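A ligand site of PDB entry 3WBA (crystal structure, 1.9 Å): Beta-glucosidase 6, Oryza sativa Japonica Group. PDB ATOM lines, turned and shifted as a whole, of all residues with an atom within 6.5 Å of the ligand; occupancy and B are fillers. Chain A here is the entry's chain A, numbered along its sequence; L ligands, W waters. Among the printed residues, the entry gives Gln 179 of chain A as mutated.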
ATOM      1  N   ALA A  29      -5.962  25.830  -4.593  1.00  0.00           N
ATOM      2  CA  ALA A  29      -6.059  24.410  -4.941  1.00  0.00           C
ATOM      3  C   ALA A  29      -7.047  23.771  -3.968  1.00  0.00           C
ATOM      4  O   ALA A  29      -7.094  24.162  -2.802  1.00  0.00           O
ATOM      5  CB  ALA A  29      -4.682  23.747  -4.824  1.00  0.00           C
ATOM      6  N   GLN A  32      -5.919  22.186  -0.497  1.00  0.00           N
ATOM      7  CA  GLN A  32      -5.344  23.207   0.391  1.00  0.00           C
ATOM      8  C   GLN A  32      -6.370  24.180   0.954  1.00  0.00           C
ATOM      9  O   GLN A  32      -6.094  24.833   1.972  1.00  0.00           O
ATOM     10  CB  GLN A  32      -4.261  23.991  -0.329  1.00  0.00           C
ATOM     11  CG  GLN A  32      -3.144  23.079  -0.925  1.00  0.00           C
ATOM     12  CD  GLN A  32      -2.061  23.915  -1.570  1.00  0.00           C
ATOM     13  OE1 GLN A  32      -2.073  24.118  -2.786  1.00  0.00           O
ATOM     14  NE2 GLN A  32      -1.120  24.396  -0.772  1.00  0.00           N
ATOM     15  N   ARG A  89      -7.874  31.236 -10.215  1.00  0.00           N
ATOM     16  CA  ARG A  89      -7.440  29.891 -10.518  1.00  0.00           C
ATOM     17  C   ARG A  89      -7.805  29.011  -9.332  1.00  0.00           C
ATOM     18  O   ARG A  89      -7.452  29.311  -8.184  1.00  0.00           O
ATOM     19  CB  ARG A  89      -5.921  29.886 -10.794  1.00  0.00           C
ATOM     20  CG  ARG A  89      -5.339  28.493 -10.970  1.00  0.00           C
ATOM     21  CD  ARG A  89      -3.966  28.452 -11.684  1.00  0.00           C
ATOM     22  NE  ARG A  89      -3.622  27.044 -11.714  1.00  0.00           N
ATOM     23  CZ  ARG A  89      -2.569  26.495 -11.134  1.00  0.00           C
ATOM     24  NH1 ARG A  89      -1.614  27.244 -10.564  1.00  0.00           N
ATOM     25  NH2 ARG A  89      -2.438  25.191 -11.179  1.00  0.00           N
ATOM     26  N   HIS A 133      -4.873  18.924  -9.235  1.00  0.00           N
ATOM     27  CA  HIS A 133      -3.893  19.543  -8.336  1.00  0.00           C
ATOM     28  C   HIS A 133      -3.546  18.592  -7.177  1.00  0.00           C
ATOM     29  O   HIS A 133      -3.690  18.945  -6.000  1.00  0.00           O
ATOM     30  CB  HIS A 133      -4.417  20.903  -7.844  1.00  0.00           C
ATOM     31  CG  HIS A 133      -3.344  21.847  -7.391  1.00  0.00           C
ATOM     32  ND1 HIS A 133      -3.184  23.097  -7.921  1.00  0.00           N
ATOM     33  CD2 HIS A 133      -2.384  21.711  -6.432  1.00  0.00           C
ATOM     34  CE1 HIS A 133      -2.165  23.707  -7.324  1.00  0.00           C
ATOM     35  NE2 HIS A 133      -1.676  22.892  -6.409  1.00  0.00           N
ATOM     36  N   TRP A 134      -3.084  17.390  -7.559  1.00  0.00           N
ATOM     37  CA  TRP A 134      -2.388  16.384  -6.698  1.00  0.00           C
ATOM     38  C   TRP A 134      -3.255  15.414  -5.916  1.00  0.00           C
ATOM     39  O   TRP A 134      -2.737  14.498  -5.281  1.00  0.00           O
ATOM     40  CB  TRP A 134      -1.369  17.027  -5.738  1.00  0.00           C
ATOM     41  CG  TRP A 134      -0.379  17.915  -6.371  1.00  0.00           C
ATOM     42  CD1 TRP A 134      -0.214  18.173  -7.720  1.00  0.00           C
ATOM     43  CD2 TRP A 134       0.592  18.698  -5.694  1.00  0.00           C
ATOM     44  NE1 TRP A 134       0.814  19.058  -7.901  1.00  0.00           N
ATOM     45  CE2 TRP A 134       1.320  19.401  -6.671  1.00  0.00           C
ATOM     46  CE3 TRP A 134       0.929  18.864  -4.337  1.00  0.00           C
ATOM     47  CZ2 TRP A 134       2.376  20.267  -6.348  1.00  0.00           C
ATOM     48  CZ3 TRP A 134       1.977  19.725  -4.004  1.00  0.00           C
ATOM     49  CH2 TRP A 134       2.691  20.411  -5.011  1.00  0.00           C
ATOM     50  N   ASN A 178      -1.304  20.297 -12.572  1.00  0.00           N
ATOM     51  CA  ASN A 178      -0.450  21.200 -11.818  1.00  0.00           C
ATOM     52  C   ASN A 178       0.888  20.563 -11.449  1.00  0.00           C
ATOM     53  O   ASN A 178       0.921  19.578 -10.702  1.00  0.00           O
ATOM     54  CB  ASN A 178      -1.151  21.655 -10.528  1.00  0.00           C
ATOM     55  CG  ASN A 178      -0.337  22.686  -9.778  1.00  0.00           C
ATOM     56  OD1 ASN A 178      -0.225  23.831 -10.215  1.00  0.00           O
ATOM     57  ND2 ASN A 178       0.274  22.276  -8.649  1.00  0.00           N
ATOM     58  N   GLN A 179       1.978  21.104 -11.988  1.00  0.00           N
ATOM     59  CA  GLN A 179       3.334  20.705 -11.598  1.00  0.00           C
ATOM     60  C   GLN A 179       3.595  19.184 -11.625  1.00  0.00           C
ATOM     61  O   GLN A 179       3.916  18.594 -10.590  1.00  0.00           O
ATOM     62  CB  GLN A 179       3.662  21.251 -10.210  1.00  0.00           C
ATOM     63  CG  GLN A 179       3.486  22.763 -10.171  1.00  0.00           C
ATOM     64  CD  GLN A 179       3.902  23.412  -8.873  1.00  0.00           C
ATOM     65  OE1 GLN A 179       3.512  24.568  -8.622  1.00  0.00           O
ATOM     66  NE2 GLN A 179       4.693  22.718  -8.049  1.00  0.00           N
ATOM     67  N   ASN A 320       4.660  28.233 -13.177  1.00  0.00           N
ATOM     68  CA  ASN A 320       4.621  28.428 -11.749  1.00  0.00           C
ATOM     69  C   ASN A 320       6.083  28.644 -11.329  1.00  0.00           C
ATOM     70  O   ASN A 320       6.887  27.718 -11.394  1.00  0.00           O
ATOM     71  CB  ASN A 320       4.092  27.190 -11.054  1.00  0.00           C
ATOM     72  CG  ASN A 320       2.590  26.962 -11.299  1.00  0.00           C
ATOM     73  OD1 ASN A 320       1.947  27.668 -12.089  1.00  0.00           O
ATOM     74  ND2 ASN A 320       2.016  25.990 -10.592  1.00  0.00           N
ATOM     75  N   TYR A 322       8.929  30.694  -8.626  1.00  0.00           N
ATOM     76  CA  TYR A 322       9.205  31.422  -7.406  1.00  0.00           C
ATOM     77  C   TYR A 322      10.635  31.961  -7.338  1.00  0.00           C
ATOM     78  O   TYR A 322      10.862  33.025  -6.793  1.00  0.00           O
ATOM     79  CB  TYR A 322       9.049  30.505  -6.203  1.00  0.00           C
ATOM     80  CG  TYR A 322       7.617  30.161  -5.913  1.00  0.00           C
ATOM     81  CD1 TYR A 322       7.108  28.926  -6.272  1.00  0.00           C
ATOM     82  CD2 TYR A 322       6.780  31.072  -5.285  1.00  0.00           C
ATOM     83  CE1 TYR A 322       5.786  28.585  -5.992  1.00  0.00           C
ATOM     84  CE2 TYR A 322       5.449  30.738  -4.999  1.00  0.00           C
ATOM     85  CZ  TYR A 322       4.968  29.510  -5.371  1.00  0.00           C
ATOM     86  OH  TYR A 322       3.650  29.166  -5.128  1.00  0.00           O
ATOM     87  N   SER A 365       9.633  29.882   3.446  1.00  0.00           N
ATOM     88  CA  SER A 365       9.998  28.571   2.933  1.00  0.00           C
ATOM     89  C   SER A 365      11.504  28.537   2.690  1.00  0.00           C
ATOM     90  O   SER A 365      12.073  29.464   2.109  1.00  0.00           O
ATOM     91  CB  SER A 365       9.218  28.235   1.659  1.00  0.00           C
ATOM     92  OG  SER A 365       7.882  27.927   1.983  1.00  0.00           O
ATOM     93  N   TRP A 367      13.280  26.931   0.765  1.00  0.00           N
ATOM     94  CA  TRP A 367      13.668  26.861  -0.658  1.00  0.00           C
ATOM     95  C   TRP A 367      13.440  28.136  -1.473  1.00  0.00           C
ATOM     96  O   TRP A 367      13.893  28.249  -2.627  1.00  0.00           O
ATOM     97  CB  TRP A 367      12.941  25.666  -1.318  1.00  0.00           C
ATOM     98  CG  TRP A 367      11.433  25.678  -1.098  1.00  0.00           C
ATOM     99  CD1 TRP A 367      10.745  25.040  -0.095  1.00  0.00           C
ATOM    100  CD2 TRP A 367      10.444  26.382  -1.886  1.00  0.00           C
ATOM    101  NE1 TRP A 367       9.394  25.305  -0.212  1.00  0.00           N
ATOM    102  CE2 TRP A 367       9.182  26.110  -1.293  1.00  0.00           C
ATOM    103  CE3 TRP A 367      10.498  27.213  -3.010  1.00  0.00           C
ATOM    104  CZ2 TRP A 367       7.979  26.648  -1.802  1.00  0.00           C
ATOM    105  CZ3 TRP A 367       9.294  27.725  -3.533  1.00  0.00           C
ATOM    106  CH2 TRP A 367       8.058  27.459  -2.908  1.00  0.00           C
ATOM    107  N   GLU A 395       1.280  30.805 -11.205  1.00  0.00           N
ATOM    108  CA  GLU A 395       1.600  30.820  -9.775  1.00  0.00           C
ATOM    109  C   GLU A 395       2.889  31.605  -9.545  1.00  0.00           C
ATOM    110  O   GLU A 395       3.901  31.306 -10.160  1.00  0.00           O
ATOM    111  CB  GLU A 395       1.810  29.366  -9.306  1.00  0.00           C
ATOM    112  CG  GLU A 395       1.796  29.189  -7.817  1.00  0.00           C
ATOM    113  CD  GLU A 395       2.551  27.945  -7.408  1.00  0.00           C
ATOM    114  OE1 GLU A 395       2.016  27.204  -6.561  1.00  0.00           O
ATOM    115  OE2 GLU A 395       3.668  27.694  -7.927  1.00  0.00           O
ATOM    116  N   TRP A 445       0.120  33.495  -5.909  1.00  0.00           N
ATOM    117  CA  TRP A 445      -0.080  32.460  -4.887  1.00  0.00           C
ATOM    118  C   TRP A 445       0.144  33.186  -3.554  1.00  0.00           C
ATOM    119  O   TRP A 445       1.257  33.645  -3.299  1.00  0.00           O
ATOM    120  CB  TRP A 445       0.910  31.280  -5.035  1.00  0.00           C
ATOM    121  CG  TRP A 445       0.496  30.189  -4.090  1.00  0.00           C
ATOM    122  CD1 TRP A 445       0.967  29.977  -2.815  1.00  0.00           C
ATOM    123  CD2 TRP A 445      -0.526  29.206  -4.321  1.00  0.00           C
ATOM    124  NE1 TRP A 445       0.285  28.926  -2.230  1.00  0.00           N
ATOM    125  CE2 TRP A 445      -0.642  28.439  -3.126  1.00  0.00           C
ATOM    126  CE3 TRP A 445      -1.384  28.921  -5.389  1.00  0.00           C
ATOM    127  CZ2 TRP A 445      -1.563  27.369  -2.986  1.00  0.00           C
ATOM    128  CZ3 TRP A 445      -2.308  27.838  -5.267  1.00  0.00           C
ATOM    129  CH2 TRP A 445      -2.385  27.093  -4.069  1.00  0.00           C
ATOM    130  N   ASN A 450      -3.189  29.117   3.597  1.00  0.00           N
ATOM    131  CA  ASN A 450      -3.859  27.844   3.403  1.00  0.00           C
ATOM    132  C   ASN A 450      -2.943  26.695   3.841  1.00  0.00           C
ATOM    133  O   ASN A 450      -1.866  26.950   4.397  1.00  0.00           O
ATOM    134  CB  ASN A 450      -4.301  27.720   1.930  1.00  0.00           C
ATOM    135  CG  ASN A 450      -3.120  27.809   0.979  1.00  0.00           C
ATOM    136  OD1 ASN A 450      -2.407  26.823   0.775  1.00  0.00           O
ATOM    137  ND2 ASN A 450      -2.867  29.007   0.437  1.00  0.00           N
ATOM    138  N   TRP A 451      -3.360  25.453   3.598  1.00  0.00           N
ATOM    139  CA  TRP A 451      -2.614  24.286   4.098  1.00  0.00           C
ATOM    140  C   TRP A 451      -1.530  23.964   3.074  1.00  0.00           C
ATOM    141  O   TRP A 451      -1.826  23.518   1.963  1.00  0.00           O
ATOM    142  CB  TRP A 451      -3.541  23.094   4.277  1.00  0.00           C
ATOM    143  CG  TRP A 451      -2.912  21.905   4.973  1.00  0.00           C
ATOM    144  CD1 TRP A 451      -2.661  21.772   6.303  1.00  0.00           C
ATOM    145  CD2 TRP A 451      -2.490  20.682   4.357  1.00  0.00           C
ATOM    146  NE1 TRP A 451      -2.116  20.533   6.563  1.00  0.00           N
ATOM    147  CE2 TRP A 451      -1.990  19.842   5.383  1.00  0.00           C
ATOM    148  CE3 TRP A 451      -2.484  20.203   3.038  1.00  0.00           C
ATOM    149  CZ2 TRP A 451      -1.488  18.563   5.146  1.00  0.00           C
ATOM    150  CZ3 TRP A 451      -1.964  18.921   2.784  1.00  0.00           C
ATOM    151  CH2 TRP A 451      -1.491  18.110   3.843  1.00  0.00           C
ATOM    152  N   GLU A 452      -0.290  24.234   3.466  1.00  0.00           N
ATOM    153  CA  GLU A 452       0.858  24.162   2.609  1.00  0.00           C
ATOM    154  C   GLU A 452       1.486  22.758   2.579  1.00  0.00           C
ATOM    155  O   GLU A 452       2.674  22.579   2.902  1.00  0.00           O
ATOM    156  CB  GLU A 452       1.874  25.251   3.025  1.00  0.00           C
ATOM    157  CG  GLU A 452       3.181  25.317   2.197  1.00  0.00           C
ATOM    158  CD  GLU A 452       2.953  25.369   0.680  1.00  0.00           C
ATOM    159  OE1 GLU A 452       1.921  25.902   0.214  1.00  0.00           O
ATOM    160  OE2 GLU A 452       3.828  24.867  -0.038  1.00  0.00           O
ATOM    161  N   TRP A 453       0.682  21.770   2.196  1.00  0.00           N
ATOM    162  CA  TRP A 453       1.169  20.413   1.956  1.00  0.00           C
ATOM    163  C   TRP A 453       1.945  19.894   3.176  1.00  0.00           C
ATOM    164  O   TRP A 453       1.436  20.026   4.276  1.00  0.00           O
ATOM    165  CB  TRP A 453       1.982  20.343   0.640  1.00  0.00           C
ATOM    166  CG  TRP A 453       1.171  20.846  -0.548  1.00  0.00           C
ATOM    167  CD1 TRP A 453       1.443  21.953  -1.304  1.00  0.00           C
ATOM    168  CD2 TRP A 453      -0.034  20.268  -1.088  1.00  0.00           C
ATOM    169  NE1 TRP A 453       0.490  22.091  -2.287  1.00  0.00           N
ATOM    170  CE2 TRP A 453      -0.432  21.085  -2.182  1.00  0.00           C
ATOM    171  CE3 TRP A 453      -0.827  19.133  -0.767  1.00  0.00           C
ATOM    172  CZ2 TRP A 453      -1.579  20.819  -2.972  1.00  0.00           C
ATOM    173  CZ3 TRP A 453      -1.961  18.850  -1.546  1.00  0.00           C
ATOM    174  CH2 TRP A 453      -2.333  19.695  -2.653  1.00  0.00           C
ATOM    175  N   SER A 459       3.202  27.785   7.067  1.00  0.00           N
ATOM    176  CA  SER A 459       3.550  28.697   5.970  1.00  0.00           C
ATOM    177  C   SER A 459       2.304  29.485   5.547  1.00  0.00           C
ATOM    178  O   SER A 459       1.257  28.894   5.323  1.00  0.00           O
ATOM    179  CB  SER A 459       4.120  27.895   4.787  1.00  0.00           C
ATOM    180  OG  SER A 459       3.960  28.596   3.557  1.00  0.00           O
ATOM    181  N   PHE A 461       1.036  31.918   2.767  1.00  0.00           N
ATOM    182  CA  PHE A 461       1.255  32.462   1.432  1.00  0.00           C
ATOM    183  C   PHE A 461       0.200  33.503   1.034  1.00  0.00           C
ATOM    184  O   PHE A 461       0.286  34.081  -0.059  1.00  0.00           O
ATOM    185  CB  PHE A 461       1.229  31.332   0.382  1.00  0.00           C
ATOM    186  CG  PHE A 461       2.567  30.697   0.107  1.00  0.00           C
ATOM    187  CD1 PHE A 461       2.939  29.517   0.735  1.00  0.00           C
ATOM    188  CD2 PHE A 461       3.447  31.282  -0.803  1.00  0.00           C
ATOM    189  CE1 PHE A 461       4.185  28.921   0.477  1.00  0.00           C
ATOM    190  CE2 PHE A 461       4.710  30.696  -1.082  1.00  0.00           C
ATOM    191  CZ  PHE A 461       5.074  29.511  -0.443  1.00  0.00           C
HETATM  192  C1  LIG L   1       2.619  26.237  -5.983  1.00  0.00           C
HETATM  193  C2  LIG L   1       1.795  24.909  -5.852  1.00  0.00           C
HETATM  194  C3  LIG L   1       0.912  25.076  -4.608  1.00  0.00           C
HETATM  195  C4  LIG L   1       1.771  25.458  -3.384  1.00  0.00           C
HETATM  196  C5  LIG L   1       2.698  26.654  -3.677  1.00  0.00           C
HETATM  197  C6  LIG L   1       3.636  26.909  -2.515  1.00  0.00           C
HETATM  198  O1  LIG L   1       1.003  24.608  -6.954  1.00  0.00           O
HETATM  199  O2  LIG L   1       0.075  24.000  -4.396  1.00  0.00           O
HETATM  200  O3  LIG L   1       1.024  25.691  -2.271  1.00  0.00           O
HETATM  201  O4  LIG L   1       3.428  26.422  -4.831  1.00  0.00           O
HETATM  202  O5  LIG L   1       4.512  25.899  -2.317  1.00  0.00           O
HETATM  203  O   HOH W   1      -0.566  26.701  -8.030  1.00  0.00           O
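Water W1 lies within hydrogen-bond range of NH1 of Arg 89 (2.8 Å), O1 of the ligand (2.8 Å) and OE1 of Glu 395 (3.0 Å).
Trp 367 touches the ligand. Phe 461 touches the ligand. Hydrophobic or aromatic side chains that line the ligand: His 133, Tyr 322, Trp 367, Trp 445, Trp 453 and Phe 461. Within 4 Å of the ligand: Gln 32, His 133, Asn 178, Gln 179, Tyr 322, Trp 367, Glu 395, Trp 445, Glu 452, Trp 453 and Phe 461. The nearest printed residue that does not touch the ligand is Asn 320 (4.02 Å).
OE1 of Glu 395 sits close to OH of Tyr 322, 2.9 Å away. The side-chain amide nitrogen of Gln 32 sits close to the indole nitrogen of Trp 453. The side-chain amide nitrogen (NE2) of Gln 32 is in hydrogen-bond range of the side-chain amide oxygen (OD1) of Asn 450. The backbone carbonyl oxygen (O) of Trp 451 sits at hydrogen-bond distance from the side-chain amide nitrogen (NE2) of Gln 32. The side-chain amide nitrogen of Asn 178 is in hydrogen-bond range of a ring nitrogen (NE2) of His 133, 3.0 Å away. The side-chain amide nitrogen of Asn 320 lies within hydrogen-bond range of the side-chain amide oxygen of Asn 178 (3.1 Å). The backbone carbonyl oxygen (O) of Asn 178 sits at hydrogen-bond distance from the indole nitrogen (NE1) of Trp 134, 2.9 Å away. The side-chain amide oxygen of Gln 179 is in hydrogen-bond range of the side-chain amide nitrogen of Asn 320 (2.9 Å).
A carbon (C1) of the ligand is covalently linked to the side-chain carboxylate (OE1) of Glu 395 (1.3 Å). An oxygen (O5) of the ligand is in hydrogen-bond range of the side-chain carboxylate (OE2) of Glu 452 (2.6 Å). An oxygen (O2) of the ligand sits at hydrogen-bond distance from the side-chain amide oxygen (OE1) of Gln 32, 2.7 Å away. The side-chain hydroxyl (OH) of Tyr 322 is in hydrogen-bond range of an oxygen (O4) of the ligand, 2.8 Å away. The indole nitrogen (NE1) of Trp 453 sits at hydrogen-bond distance from an oxygen (O2) of the ligand (2.9 Å). An oxygen (O2) of the ligand lies within hydrogen-bond range of a ring nitrogen (NE2) of His 133 (2.9 Å). ND2 of Asn 178 is in hydrogen-bond range of O1 of the ligand (3.0 Å). The side-chain amide oxygen (OE1) of Gln 179 is in hydrogen-bond range of an oxygen (O1) of the ligand, at 3.0 Å. An oxygen (O3) of the ligand sits close to the indole nitrogen (NE1) of Trp 445, at 3.3 Å.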
